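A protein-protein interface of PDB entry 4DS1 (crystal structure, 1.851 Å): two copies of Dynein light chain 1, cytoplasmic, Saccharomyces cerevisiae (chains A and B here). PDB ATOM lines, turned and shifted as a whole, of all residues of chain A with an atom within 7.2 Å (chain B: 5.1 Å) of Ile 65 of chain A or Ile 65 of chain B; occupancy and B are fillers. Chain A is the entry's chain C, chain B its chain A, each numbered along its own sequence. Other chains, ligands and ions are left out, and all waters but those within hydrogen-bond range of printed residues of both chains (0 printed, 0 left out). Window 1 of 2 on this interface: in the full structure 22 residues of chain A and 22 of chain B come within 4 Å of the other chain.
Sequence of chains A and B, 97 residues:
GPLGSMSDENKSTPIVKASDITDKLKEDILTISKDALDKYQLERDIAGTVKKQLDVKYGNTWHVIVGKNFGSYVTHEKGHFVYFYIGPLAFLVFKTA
The backbone carbonyl oxygen (O) of Val 64 of chain B is in hydrogen-bond range of the backbone NH (N) of Tyr 73 of chain A, at 3.0 Å.
The backbone carbonyl oxygen (O) of Val 66 of chain B is in hydrogen-bond range of the backbone NH (N) of Gly 71 of chain A (2.7 Å).
The side-chain carboxylate of Glu 43 of chain A sits close to the backbone NH of Phe 70 of chain B (3.4 Å).
The backbone NH (N) of Gly 71 of chain B is in hydrogen-bond range of the side-chain carboxylate (OE1) of Glu 43 of chain A (3.4 Å).
N of Gly 71 of chain B sits at hydrogen-bond distance from O of Val 66 of chain A (2.7 Å).
OG of Ser 72 of chain B is in hydrogen-bond range of O of Val 64 of chain A (3.1 Å).
The backbone NH (N) of Leu 92 of chain B lies within hydrogen-bond range of the backbone carbonyl oxygen (O) of Ile 65 of chain B, at 2.8 Å.
O of Gly 67 of chain B is in hydrogen-bond range of N of Ala 90 of chain B (2.8 Å).
The backbone NH of His 63 of chain A sits at hydrogen-bond distance from the backbone carbonyl oxygen of Phe 94 of chain A (2.9 Å).
The backbone NH (N) of Leu 92 of chain A sits at hydrogen-bond distance from the backbone carbonyl oxygen (O) of Ile 65 of chain A (2.9 Å).
N of Ala 90 of chain A is in hydrogen-bond range of O of Gly 67 of chain A (2.8 Å).
Among the printed residues, pairs that only touch across the chains: Ala 47 of chain A with Ser 72 of chain B, His 63 of chain A with Val 74 of chain B, Ile 65 of chain A with Ile 65 of chain B, Ile 65 of chain A with Gly 71 of chain B, Ile 65 of chain A with Ser 72 of chain B, Val 66 of chain A with Phe 70 of chain B, Gly 67 of chain A with Phe 70 of chain B, Asn 69 of chain A with Gly 67 of chain B, Phe 70 of chain A with Ile 65 of chain B, Phe 70 of chain A with Val 66 of chain B, Phe 70 of chain A with Gly 67 of chain B, Phe 70 of chain A with Phe 70 of chain B, Gly 71 of chain A with Ile 65 of chain B, Ser 72 of chain A with Val 64 of chain B, Ser 72 of chain A with Ile 65 of chain B, Tyr 73 of chain A with Ala 47 of chain B, Tyr 73 of chain A with His 63 of chain B, Val 74 of chain A with His 63 of chain B and Phe 94 of chain A with His 63 of chain B.
Of chain B, only Ile 65 (3.9 Å), Gly 71 (3.5 Å) and Ser 72 (3.5 Å) come within 4 Å of Ile 65 of chain A.
Ile 65 of chain B touches four residues of chain A.
Printed residues of chain A within 4 Å of Gly 71 of chain B: Glu 43, Ile 65 and Val 66.
Of the printed residues of chain A, Val 74 of chain B touches His 63.
Of the printed residues of chain B, Val 74 of chain A touches His 63.
Of the printed residues of chain A, Phe 70 of chain B touches Glu 43 (3.2 Å), Val 66 (3.3 Å), Gly 67 (3.8 Å) and Phe 70 (3.9 Å).
Phe 91 of chain A touches none of the printed residues of chain B.
Tyr 83 of chain A touches none of the printed residues of chain B.
The nearest residue of chain B that does not touch Ile 65 of chain A is Phe 70 of chain B (4.03 Å).
The nearest residue of chain A that does not touch Ile 65 of chain B is Val 74 of chain A (4.2 Å).
The nearest printed residue of chain B that does not touch Val 66 of chain A is Ser 72 of chain B (4.9 Å).
Hydrophobic or aromatic side chains of chain A within 4 Å of the printed part of chain B: Ala 47, His 63, Ile 65, Phe 70, Tyr 73, Val 74 and Phe 94.
Of the 13 printed residues of chain B, 10 touch a printed residue of chain A.
Ile 65 of chain A touches Gly 71 of chain B, and with the chains exchanged Gly 71 of chain A touches Ile 65 of chain B.
Ile 65 of chain A touches Ser 72 of chain B, and with the chains exchanged Ser 72 of chain A touches Ile 65 of chain B.
Gly 67 of chain A touches Phe 70 of chain B, and with the chains exchanged Phe 70 of chain A touches Gly 67 of chain B.
Phe 70 of chain A touches its own counterpart, Phe 70 of chain B.
13 positions are printed for both chains.
Of the 25 pairs that touch across the chains among the printed residues, 16 have their exchanged pair printed and touching as well.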
ATOM      1  N   GLU A  43      17.048  19.405 -18.548  1.00  0.00           N
ATOM      2  CA  GLU A  43      16.105  18.330 -18.847  1.00  0.00           C
ATOM      3  C   GLU A  43      16.726  17.256 -19.745  1.00  0.00           C
ATOM      4  O   GLU A  43      16.526  16.065 -19.524  1.00  0.00           O
ATOM      5  CB  GLU A  43      14.814  18.901 -19.460  1.00  0.00           C
ATOM      6  CG  GLU A  43      13.916  19.584 -18.424  1.00  0.00           C
ATOM      7  CD  GLU A  43      12.938  20.582 -19.038  1.00  0.00           C
ATOM      8  OE1 GLU A  43      13.032  20.846 -20.259  1.00  0.00           O
ATOM      9  OE2 GLU A  43      12.067  21.105 -18.300  1.00  0.00           O
ATOM     10  N   ALA A  47      17.135  13.293 -18.864  1.00  0.00           N
ATOM     11  CA  ALA A  47      16.544  12.292 -19.755  1.00  0.00           C
ATOM     12  C   ALA A  47      17.595  11.317 -20.260  1.00  0.00           C
ATOM     13  O   ALA A  47      17.360  10.106 -20.325  1.00  0.00           O
ATOM     14  CB  ALA A  47      15.845  12.972 -20.933  1.00  0.00           C
ATOM     15  N   HIS A  63      13.166   5.245 -24.086  1.00  0.00           N
ATOM     16  CA  HIS A  63      13.044   6.621 -24.542  1.00  0.00           C
ATOM     17  C   HIS A  63      12.540   7.434 -23.367  1.00  0.00           C
ATOM     18  O   HIS A  63      11.647   6.990 -22.643  1.00  0.00           O
ATOM     19  CB  HIS A  63      12.047   6.713 -25.694  1.00  0.00           C
ATOM     20  CG  HIS A  63      12.275   5.698 -26.767  1.00  0.00           C
ATOM     21  ND1 HIS A  63      13.072   5.939 -27.870  1.00  0.00           N
ATOM     22  CD2 HIS A  63      11.823   4.428 -26.898  1.00  0.00           C
ATOM     23  CE1 HIS A  63      13.092   4.862 -28.636  1.00  0.00           C
ATOM     24  NE2 HIS A  63      12.344   3.932 -28.067  1.00  0.00           N
ATOM     25  N   VAL A  64      13.108   8.616 -23.168  1.00  0.00           N
ATOM     26  CA  VAL A  64      12.772   9.402 -21.990  1.00  0.00           C
ATOM     27  C   VAL A  64      12.536  10.849 -22.366  1.00  0.00           C
ATOM     28  O   VAL A  64      13.346  11.444 -23.071  1.00  0.00           O
ATOM     29  CB  VAL A  64      13.877   9.341 -20.915  1.00  0.00           C
ATOM     30  CG1 VAL A  64      13.499  10.227 -19.724  1.00  0.00           C
ATOM     31  CG2 VAL A  64      14.104   7.901 -20.473  1.00  0.00           C
ATOM     32  N   ILE A  65      11.414  11.398 -21.904  1.00  0.00           N
ATOM     33  CA  ILE A  65      11.099  12.817 -22.089  1.00  0.00           C
ATOM     34  C   ILE A  65      10.931  13.434 -20.693  1.00  0.00           C
ATOM     35  O   ILE A  65      10.240  12.871 -19.860  1.00  0.00           O
ATOM     36  CB  ILE A  65       9.800  13.025 -22.926  1.00  0.00           C
ATOM     37  CG1 ILE A  65       9.983  12.505 -24.355  1.00  0.00           C
ATOM     38  CG2 ILE A  65       9.419  14.505 -22.970  1.00  0.00           C
ATOM     39  CD1 ILE A  65      10.053  10.999 -24.480  1.00  0.00           C
ATOM     40  N   VAL A  66      11.605  14.554 -20.428  1.00  0.00           N
ATOM     41  CA  VAL A  66      11.503  15.237 -19.133  1.00  0.00           C
ATOM     42  C   VAL A  66      11.182  16.701 -19.397  1.00  0.00           C
ATOM     43  O   VAL A  66      11.888  17.367 -20.152  1.00  0.00           O
ATOM     44  CB  VAL A  66      12.832  15.151 -18.340  1.00  0.00           C
ATOM     45  CG1 VAL A  66      12.704  15.832 -16.977  1.00  0.00           C
ATOM     46  CG2 VAL A  66      13.266  13.698 -18.171  1.00  0.00           C
ATOM     47  N   GLY A  67      10.123  17.217 -18.786  1.00  0.00           N
ATOM     48  CA  GLY A  67       9.734  18.588 -19.075  1.00  0.00           C
ATOM     49  C   GLY A  67       8.514  19.077 -18.332  1.00  0.00           C
ATOM     50  O   GLY A  67       7.845  18.304 -17.649  1.00  0.00           O
ATOM     51  N   ASN A  69       6.191  21.219 -20.064  1.00  0.00           N
ATOM     52  CA  ASN A  69       5.131  21.430 -21.034  1.00  0.00           C
ATOM     53  C   ASN A  69       5.320  20.640 -22.307  1.00  0.00           C
ATOM     54  O   ASN A  69       6.101  21.027 -23.179  1.00  0.00           O
ATOM     55  CB  ASN A  69       4.965  22.905 -21.395  1.00  0.00           C
ATOM     56  CG  ASN A  69       3.922  23.112 -22.475  1.00  0.00           C
ATOM     57  OD1 ASN A  69       4.251  23.261 -23.652  1.00  0.00           O
ATOM     58  ND2 ASN A  69       2.650  23.080 -22.087  1.00  0.00           N
ATOM     59  N   PHE A  70       4.590  19.539 -22.414  1.00  0.00           N
ATOM     60  CA  PHE A  70       4.555  18.783 -23.661  1.00  0.00           C
ATOM     61  C   PHE A  70       3.313  17.907 -23.728  1.00  0.00           C
ATOM     62  O   PHE A  70       2.708  17.596 -22.707  1.00  0.00           O
ATOM     63  CB  PHE A  70       5.828  17.936 -23.841  1.00  0.00           C
ATOM     64  CG  PHE A  70       6.030  16.876 -22.782  1.00  0.00           C
ATOM     65  CD1 PHE A  70       5.494  15.600 -22.940  1.00  0.00           C
ATOM     66  CD2 PHE A  70       6.774  17.145 -21.645  1.00  0.00           C
ATOM     67  CE1 PHE A  70       5.687  14.621 -21.967  1.00  0.00           C
ATOM     68  CE2 PHE A  70       6.980  16.173 -20.669  1.00  0.00           C
ATOM     69  CZ  PHE A  70       6.435  14.906 -20.832  1.00  0.00           C
ATOM     70  N   GLY A  71       2.928  17.556 -24.949  1.00  0.00           N
ATOM     71  CA  GLY A  71       1.967  16.499 -25.179  1.00  0.00           C
ATOM     72  C   GLY A  71       2.682  15.412 -25.954  1.00  0.00           C
ATOM     73  O   GLY A  71       3.568  15.694 -26.757  1.00  0.00           O
ATOM     74  N   SER A  72       2.299  14.166 -25.725  1.00  0.00           N
ATOM     75  CA  SER A  72       2.984  13.073 -26.387  1.00  0.00           C
ATOM     76  C   SER A  72       2.028  11.989 -26.844  1.00  0.00           C
ATOM     77  O   SER A  72       0.997  11.742 -26.227  1.00  0.00           O
ATOM     78  CB  SER A  72       4.029  12.470 -25.450  1.00  0.00           C
ATOM     79  OG  SER A  72       3.411  11.963 -24.276  1.00  0.00           O
ATOM     80  N   TYR A  73       2.378  11.341 -27.944  1.00  0.00           N
ATOM     81  CA  TYR A  73       1.633  10.189 -28.383  1.00  0.00           C
ATOM     82  C   TYR A  73       2.642   9.175 -28.904  1.00  0.00           C
ATOM     83  O   TYR A  73       3.335   9.420 -29.893  1.00  0.00           O
ATOM     84  CB  TYR A  73       0.619  10.570 -29.459  1.00  0.00           C
ATOM     85  CG  TYR A  73      -0.483   9.550 -29.559  1.00  0.00           C
ATOM     86  CD1 TYR A  73      -1.694   9.745 -28.906  1.00  0.00           C
ATOM     87  CD2 TYR A  73      -0.292   8.364 -30.258  1.00  0.00           C
ATOM     88  CE1 TYR A  73      -2.700   8.801 -28.968  1.00  0.00           C
ATOM     89  CE2 TYR A  73      -1.302   7.410 -30.330  1.00  0.00           C
ATOM     90  CZ  TYR A  73      -2.497   7.635 -29.675  1.00  0.00           C
ATOM     91  OH  TYR A  73      -3.498   6.689 -29.756  1.00  0.00           O
ATOM     92  N   VAL A  74       2.742   8.051 -28.204  1.00  0.00           N
ATOM     93  CA  VAL A  74       3.779   7.075 -28.484  1.00  0.00           C
ATOM     94  C   VAL A  74       3.211   5.661 -28.431  1.00  0.00           C
ATOM     95  O   VAL A  74       2.073   5.445 -28.001  1.00  0.00           O
ATOM     96  CB  VAL A  74       4.957   7.193 -27.473  1.00  0.00           C
ATOM     97  CG1 VAL A  74       5.470   8.644 -27.399  1.00  0.00           C
ATOM     98  CG2 VAL A  74       4.527   6.704 -26.096  1.00  0.00           C
ATOM     99  N   TYR A  83       4.466   7.329 -16.546  1.00  0.00           N
ATOM    100  CA  TYR A  83       4.461   8.772 -16.707  1.00  0.00           C
ATOM    101  C   TYR A  83       4.209   9.342 -15.335  1.00  0.00           C
ATOM    102  O   TYR A  83       3.214   8.999 -14.691  1.00  0.00           O
ATOM    103  CB  TYR A  83       3.363   9.196 -17.677  1.00  0.00           C
ATOM    104  CG  TYR A  83       3.066  10.686 -17.654  1.00  0.00           C
ATOM    105  CD1 TYR A  83       3.991  11.610 -18.126  1.00  0.00           C
ATOM    106  CD2 TYR A  83       1.855  11.165 -17.170  1.00  0.00           C
ATOM    107  CE1 TYR A  83       3.716  12.973 -18.107  1.00  0.00           C
ATOM    108  CE2 TYR A  83       1.573  12.519 -17.144  1.00  0.00           C
ATOM    109  CZ  TYR A  83       2.509  13.417 -17.614  1.00  0.00           C
ATOM    110  OH  TYR A  83       2.219  14.764 -17.596  1.00  0.00           O
ATOM    111  N   PHE A  84       5.125  10.184 -14.871  1.00  0.00           N
ATOM    112  CA  PHE A  84       5.110  10.634 -13.484  1.00  0.00           C
ATOM    113  C   PHE A  84       5.750  12.006 -13.329  1.00  0.00           C
ATOM    114  O   PHE A  84       6.555  12.426 -14.159  1.00  0.00           O
ATOM    115  CB  PHE A  84       5.826   9.621 -12.580  1.00  0.00           C
ATOM    116  CG  PHE A  84       7.288   9.406 -12.926  1.00  0.00           C
ATOM    117  CD1 PHE A  84       7.655   8.489 -13.898  1.00  0.00           C
ATOM    118  CD2 PHE A  84       8.287  10.113 -12.267  1.00  0.00           C
ATOM    119  CE1 PHE A  84       8.991   8.281 -14.220  1.00  0.00           C
ATOM    120  CE2 PHE A  84       9.620   9.909 -12.584  1.00  0.00           C
ATOM    121  CZ  PHE A  84       9.971   8.986 -13.560  1.00  0.00           C
ATOM    122  N   LEU A  89       8.573  18.642 -12.615  1.00  0.00           N
ATOM    123  CA  LEU A  89       8.991  17.974 -13.844  1.00  0.00           C
ATOM    124  C   LEU A  89       8.204  16.708 -14.159  1.00  0.00           C
ATOM    125  O   LEU A  89       8.149  15.789 -13.348  1.00  0.00           O
ATOM    126  CB  LEU A  89      10.483  17.626 -13.800  1.00  0.00           C
ATOM    127  CG  LEU A  89      11.481  18.789 -13.816  1.00  0.00           C
ATOM    128  CD1 LEU A  89      12.905  18.293 -13.561  1.00  0.00           C
ATOM    129  CD2 LEU A  89      11.404  19.516 -15.137  1.00  0.00           C
ATOM    130  N   ALA A  90       7.639  16.656 -15.361  1.00  0.00           N
ATOM    131  CA  ALA A  90       6.989  15.440 -15.848  1.00  0.00           C
ATOM    132  C   ALA A  90       8.016  14.526 -16.514  1.00  0.00           C
ATOM    133  O   ALA A  90       8.876  14.998 -17.257  1.00  0.00           O
ATOM    134  CB  ALA A  90       5.883  15.791 -16.831  1.00  0.00           C
ATOM    135  N   PHE A  91       7.918  13.225 -16.244  1.00  0.00           N
ATOM    136  CA  PHE A  91       8.780  12.220 -16.858  1.00  0.00           C
ATOM    137  C   PHE A  91       7.914  11.245 -17.647  1.00  0.00           C
ATOM    138  O   PHE A  91       6.981  10.656 -17.097  1.00  0.00           O
ATOM    139  CB  PHE A  91       9.523  11.399 -15.797  1.00  0.00           C
ATOM    140  CG  PHE A  91      10.628  12.141 -15.080  1.00  0.00           C
ATOM    141  CD1 PHE A  91      10.341  13.180 -14.201  1.00  0.00           C
ATOM    142  CD2 PHE A  91      11.952  11.753 -15.240  1.00  0.00           C
ATOM    143  CE1 PHE A  91      11.363  13.839 -13.517  1.00  0.00           C
ATOM    144  CE2 PHE A  91      12.991  12.424 -14.563  1.00  0.00           C
ATOM    145  CZ  PHE A  91      12.688  13.457 -13.696  1.00  0.00           C
ATOM    146  N   LEU A  92       8.223  11.076 -18.928  1.00  0.00           N
ATOM    147  CA  LEU A  92       7.611  10.026 -19.735  1.00  0.00           C
ATOM    148  C   LEU A  92       8.720   9.035 -20.061  1.00  0.00           C
ATOM    149  O   LEU A  92       9.744   9.409 -20.648  1.00  0.00           O
ATOM    150  CB  LEU A  92       7.012  10.605 -21.018  1.00  0.00           C
ATOM    151  CG  LEU A  92       6.698   9.612 -22.147  1.00  0.00           C
ATOM    152  CD1 LEU A  92       5.662   8.582 -21.697  1.00  0.00           C
ATOM    153  CD2 LEU A  92       6.191  10.377 -23.367  1.00  0.00           C
ATOM    154  N   VAL A  93       8.543   7.782 -19.639  1.00  0.00           N
ATOM    155  CA  VAL A  93       9.591   6.769 -19.786  1.00  0.00           C
ATOM    156  C   VAL A  93       8.969   5.526 -20.390  1.00  0.00           C
ATOM    157  O   VAL A  93       8.007   4.980 -19.838  1.00  0.00           O
ATOM    158  CB  VAL A  93      10.202   6.398 -18.424  1.00  0.00           C
ATOM    159  CG1 VAL A  93      11.248   5.283 -18.583  1.00  0.00           C
ATOM    160  CG2 VAL A  93      10.832   7.613 -17.770  1.00  0.00           C
ATOM    161  N   PHE A  94       9.482   5.071 -21.521  1.00  0.00           N
ATOM    162  CA  PHE A  94       8.885   3.883 -22.131  1.00  0.00           C
ATOM    163  C   PHE A  94       9.860   3.115 -22.997  1.00  0.00           C
ATOM    164  O   PHE A  94      10.892   3.649 -23.421  1.00  0.00           O
ATOM    165  CB  PHE A  94       7.631   4.254 -22.933  1.00  0.00           C
ATOM    166  CG  PHE A  94       7.910   5.094 -24.152  1.00  0.00           C
ATOM    167  CD1 PHE A  94       8.160   6.452 -24.033  1.00  0.00           C
ATOM    168  CD2 PHE A  94       7.903   4.523 -25.417  1.00  0.00           C
ATOM    169  CE1 PHE A  94       8.403   7.226 -25.152  1.00  0.00           C
ATOM    170  CE2 PHE A  94       8.150   5.290 -26.546  1.00  0.00           C
ATOM    171  CZ  PHE A  94       8.399   6.645 -26.411  1.00  0.00           C
ATOM    172  N   ALA B  47       0.200  15.833 -31.460  1.00  0.00           N
ATOM    173  CA  ALA B  47       1.178  14.747 -31.540  1.00  0.00           C
ATOM    174  C   ALA B  47       0.475  13.476 -32.013  1.00  0.00           C
ATOM    175  O   ALA B  47       0.990  12.729 -32.857  1.00  0.00           O
ATOM    176  CB  ALA B  47       1.847  14.523 -30.183  1.00  0.00           C
ATOM    177  N   HIS B  63       6.622   8.000 -33.119  1.00  0.00           N
ATOM    178  CA  HIS B  63       6.428   8.578 -31.793  1.00  0.00           C
ATOM    179  C   HIS B  63       6.565  10.072 -31.945  1.00  0.00           C
ATOM    180  O   HIS B  63       7.450  10.540 -32.657  1.00  0.00           O
ATOM    181  CB  HIS B  63       7.487   8.053 -30.822  1.00  0.00           C
ATOM    182  CG  HIS B  63       7.661   6.568 -30.881  1.00  0.00           C
ATOM    183  ND1 HIS B  63       6.935   5.700 -30.092  1.00  0.00           N
ATOM    184  CD2 HIS B  63       8.471   5.798 -31.645  1.00  0.00           C
ATOM    185  CE1 HIS B  63       7.289   4.456 -30.373  1.00  0.00           C
ATOM    186  NE2 HIS B  63       8.226   4.488 -31.303  1.00  0.00           N
ATOM    187  N   VAL B  64       5.688  10.823 -31.301  1.00  0.00           N
ATOM    188  CA  VAL B  64       5.693  12.273 -31.470  1.00  0.00           C
ATOM    189  C   VAL B  64       5.551  12.997 -30.138  1.00  0.00           C
ATOM    190  O   VAL B  64       4.703  12.647 -29.312  1.00  0.00           O
ATOM    191  CB  VAL B  64       4.586  12.723 -32.446  1.00  0.00           C
ATOM    192  CG1 VAL B  64       4.566  14.241 -32.561  1.00  0.00           C
ATOM    193  CG2 VAL B  64       4.793  12.084 -33.825  1.00  0.00           C
ATOM    194  N   ILE B  65       6.413  13.992 -29.922  1.00  0.00           N
ATOM    195  CA  ILE B  65       6.319  14.873 -28.765  1.00  0.00           C
ATOM    196  C   ILE B  65       6.155  16.307 -29.274  1.00  0.00           C
ATOM    197  O   ILE B  65       6.892  16.742 -30.152  1.00  0.00           O
ATOM    198  CB  ILE B  65       7.584  14.826 -27.876  1.00  0.00           C
ATOM    199  CG1 ILE B  65       8.047  13.387 -27.624  1.00  0.00           C
ATOM    200  CG2 ILE B  65       7.362  15.625 -26.571  1.00  0.00           C
ATOM    201  CD1 ILE B  65       7.037  12.488 -26.956  1.00  0.00           C
ATOM    202  N   VAL B  66       5.184  17.033 -28.725  1.00  0.00           N
ATOM    203  CA  VAL B  66       4.938  18.418 -29.124  1.00  0.00           C
ATOM    204  C   VAL B  66       4.860  19.262 -27.871  1.00  0.00           C
ATOM    205  O   VAL B  66       4.032  18.992 -27.008  1.00  0.00           O
ATOM    206  CB  VAL B  66       3.587  18.550 -29.844  1.00  0.00           C
ATOM    207  CG1 VAL B  66       3.291  20.023 -30.165  1.00  0.00           C
ATOM    208  CG2 VAL B  66       3.556  17.683 -31.104  1.00  0.00           C
ATOM    209  N   GLY B  67       5.708  20.282 -27.744  1.00  0.00           N
ATOM    210  CA  GLY B  67       5.667  21.097 -26.539  1.00  0.00           C
ATOM    211  C   GLY B  67       6.589  22.299 -26.546  1.00  0.00           C
ATOM    212  O   GLY B  67       7.346  22.485 -27.490  1.00  0.00           O
ATOM    213  N   PHE B  70      10.739  20.855 -22.820  1.00  0.00           N
ATOM    214  CA  PHE B  70      11.146  19.496 -22.505  1.00  0.00           C
ATOM    215  C   PHE B  70      12.536  19.210 -23.036  1.00  0.00           C
ATOM    216  O   PHE B  70      12.999  19.848 -23.989  1.00  0.00           O
ATOM    217  CB  PHE B  70      10.141  18.472 -23.065  1.00  0.00           C
ATOM    218  CG  PHE B  70      10.030  18.464 -24.575  1.00  0.00           C
ATOM    219  CD1 PHE B  70      10.712  17.519 -25.333  1.00  0.00           C
ATOM    220  CD2 PHE B  70       9.201  19.362 -25.230  1.00  0.00           C
ATOM    221  CE1 PHE B  70      10.598  17.502 -26.719  1.00  0.00           C
ATOM    222  CE2 PHE B  70       9.086  19.353 -26.613  1.00  0.00           C
ATOM    223  CZ  PHE B  70       9.782  18.415 -27.358  1.00  0.00           C
ATOM    224  N   GLY B  71      13.198  18.253 -22.395  1.00  0.00           N
ATOM    225  CA  GLY B  71      14.427  17.657 -22.900  1.00  0.00           C
ATOM    226  C   GLY B  71      14.111  16.197 -23.149  1.00  0.00           C
ATOM    227  O   GLY B  71      13.194  15.642 -22.529  1.00  0.00           O
ATOM    228  N   SER B  72      14.832  15.567 -24.066  1.00  0.00           N
ATOM    229  CA  SER B  72      14.520  14.186 -24.399  1.00  0.00           C
ATOM    230  C   SER B  72      15.747  13.440 -24.886  1.00  0.00           C
ATOM    231  O   SER B  72      16.637  14.026 -25.491  1.00  0.00           O
ATOM    232  CB  SER B  72      13.441  14.138 -25.483  1.00  0.00           C
ATOM    233  OG  SER B  72      13.117  12.795 -25.828  1.00  0.00           O
ATOM    234  N   VAL B  74      16.180   9.833 -27.040  1.00  0.00           N
ATOM    235  CA  VAL B  74      15.459   8.755 -27.701  1.00  0.00           C
ATOM    236  C   VAL B  74      16.373   8.017 -28.665  1.00  0.00           C
ATOM    237  O   VAL B  74      17.499   8.447 -28.937  1.00  0.00           O
ATOM    238  CB  VAL B  74      14.245   9.278 -28.497  1.00  0.00           C
ATOM    239  CG1 VAL B  74      13.358  10.134 -27.602  1.00  0.00           C
ATOM    240  CG2 VAL B  74      14.713  10.081 -29.724  1.00  0.00           C
ATOM    241  N   ALA B  90       7.757  23.253 -30.200  1.00  0.00           N
ATOM    242  CA  ALA B  90       8.737  22.267 -30.648  1.00  0.00           C
ATOM    243  C   ALA B  90       8.085  20.927 -31.001  1.00  0.00           C
ATOM    244  O   ALA B  90       7.165  20.472 -30.318  1.00  0.00           O
ATOM    245  CB  ALA B  90       9.808  22.061 -29.589  1.00  0.00           C
ATOM    246  N   PHE B  91       8.577  20.301 -32.061  1.00  0.00           N
ATOM    247  CA  PHE B  91       8.100  18.990 -32.495  1.00  0.00           C
ATOM    248  C   PHE B  91       9.260  17.998 -32.544  1.00  0.00           C
ATOM    249  O   PHE B  91      10.253  18.247 -33.236  1.00  0.00           O
ATOM    250  CB  PHE B  91       7.536  19.069 -33.918  1.00  0.00           C
ATOM    251  CG  PHE B  91       6.208  19.771 -34.032  1.00  0.00           C
ATOM    252  CD1 PHE B  91       6.113  21.142 -33.888  1.00  0.00           C
ATOM    253  CD2 PHE B  91       5.060  19.049 -34.340  1.00  0.00           C
ATOM    254  CE1 PHE B  91       4.891  21.785 -34.019  1.00  0.00           C
ATOM    255  CE2 PHE B  91       3.837  19.685 -34.467  1.00  0.00           C
ATOM    256  CZ  PHE B  91       3.751  21.056 -34.302  1.00  0.00           C
ATOM    257  N   LEU B  92       9.120  16.868 -31.850  1.00  0.00           N
ATOM    258  CA  LEU B  92      10.083  15.766 -31.965  1.00  0.00           C
ATOM    259  C   LEU B  92       9.353  14.597 -32.620  1.00  0.00           C
ATOM    260  O   LEU B  92       8.378  14.081 -32.070  1.00  0.00           O
ATOM    261  CB  LEU B  92      10.619  15.379 -30.576  1.00  0.00           C
ATOM    262  CG  LEU B  92      11.421  14.086 -30.380  1.00  0.00           C
ATOM    263  CD1 LEU B  92      12.637  14.067 -31.274  1.00  0.00           C
ATOM    264  CD2 LEU B  92      11.826  13.923 -28.912  1.00  0.00           C
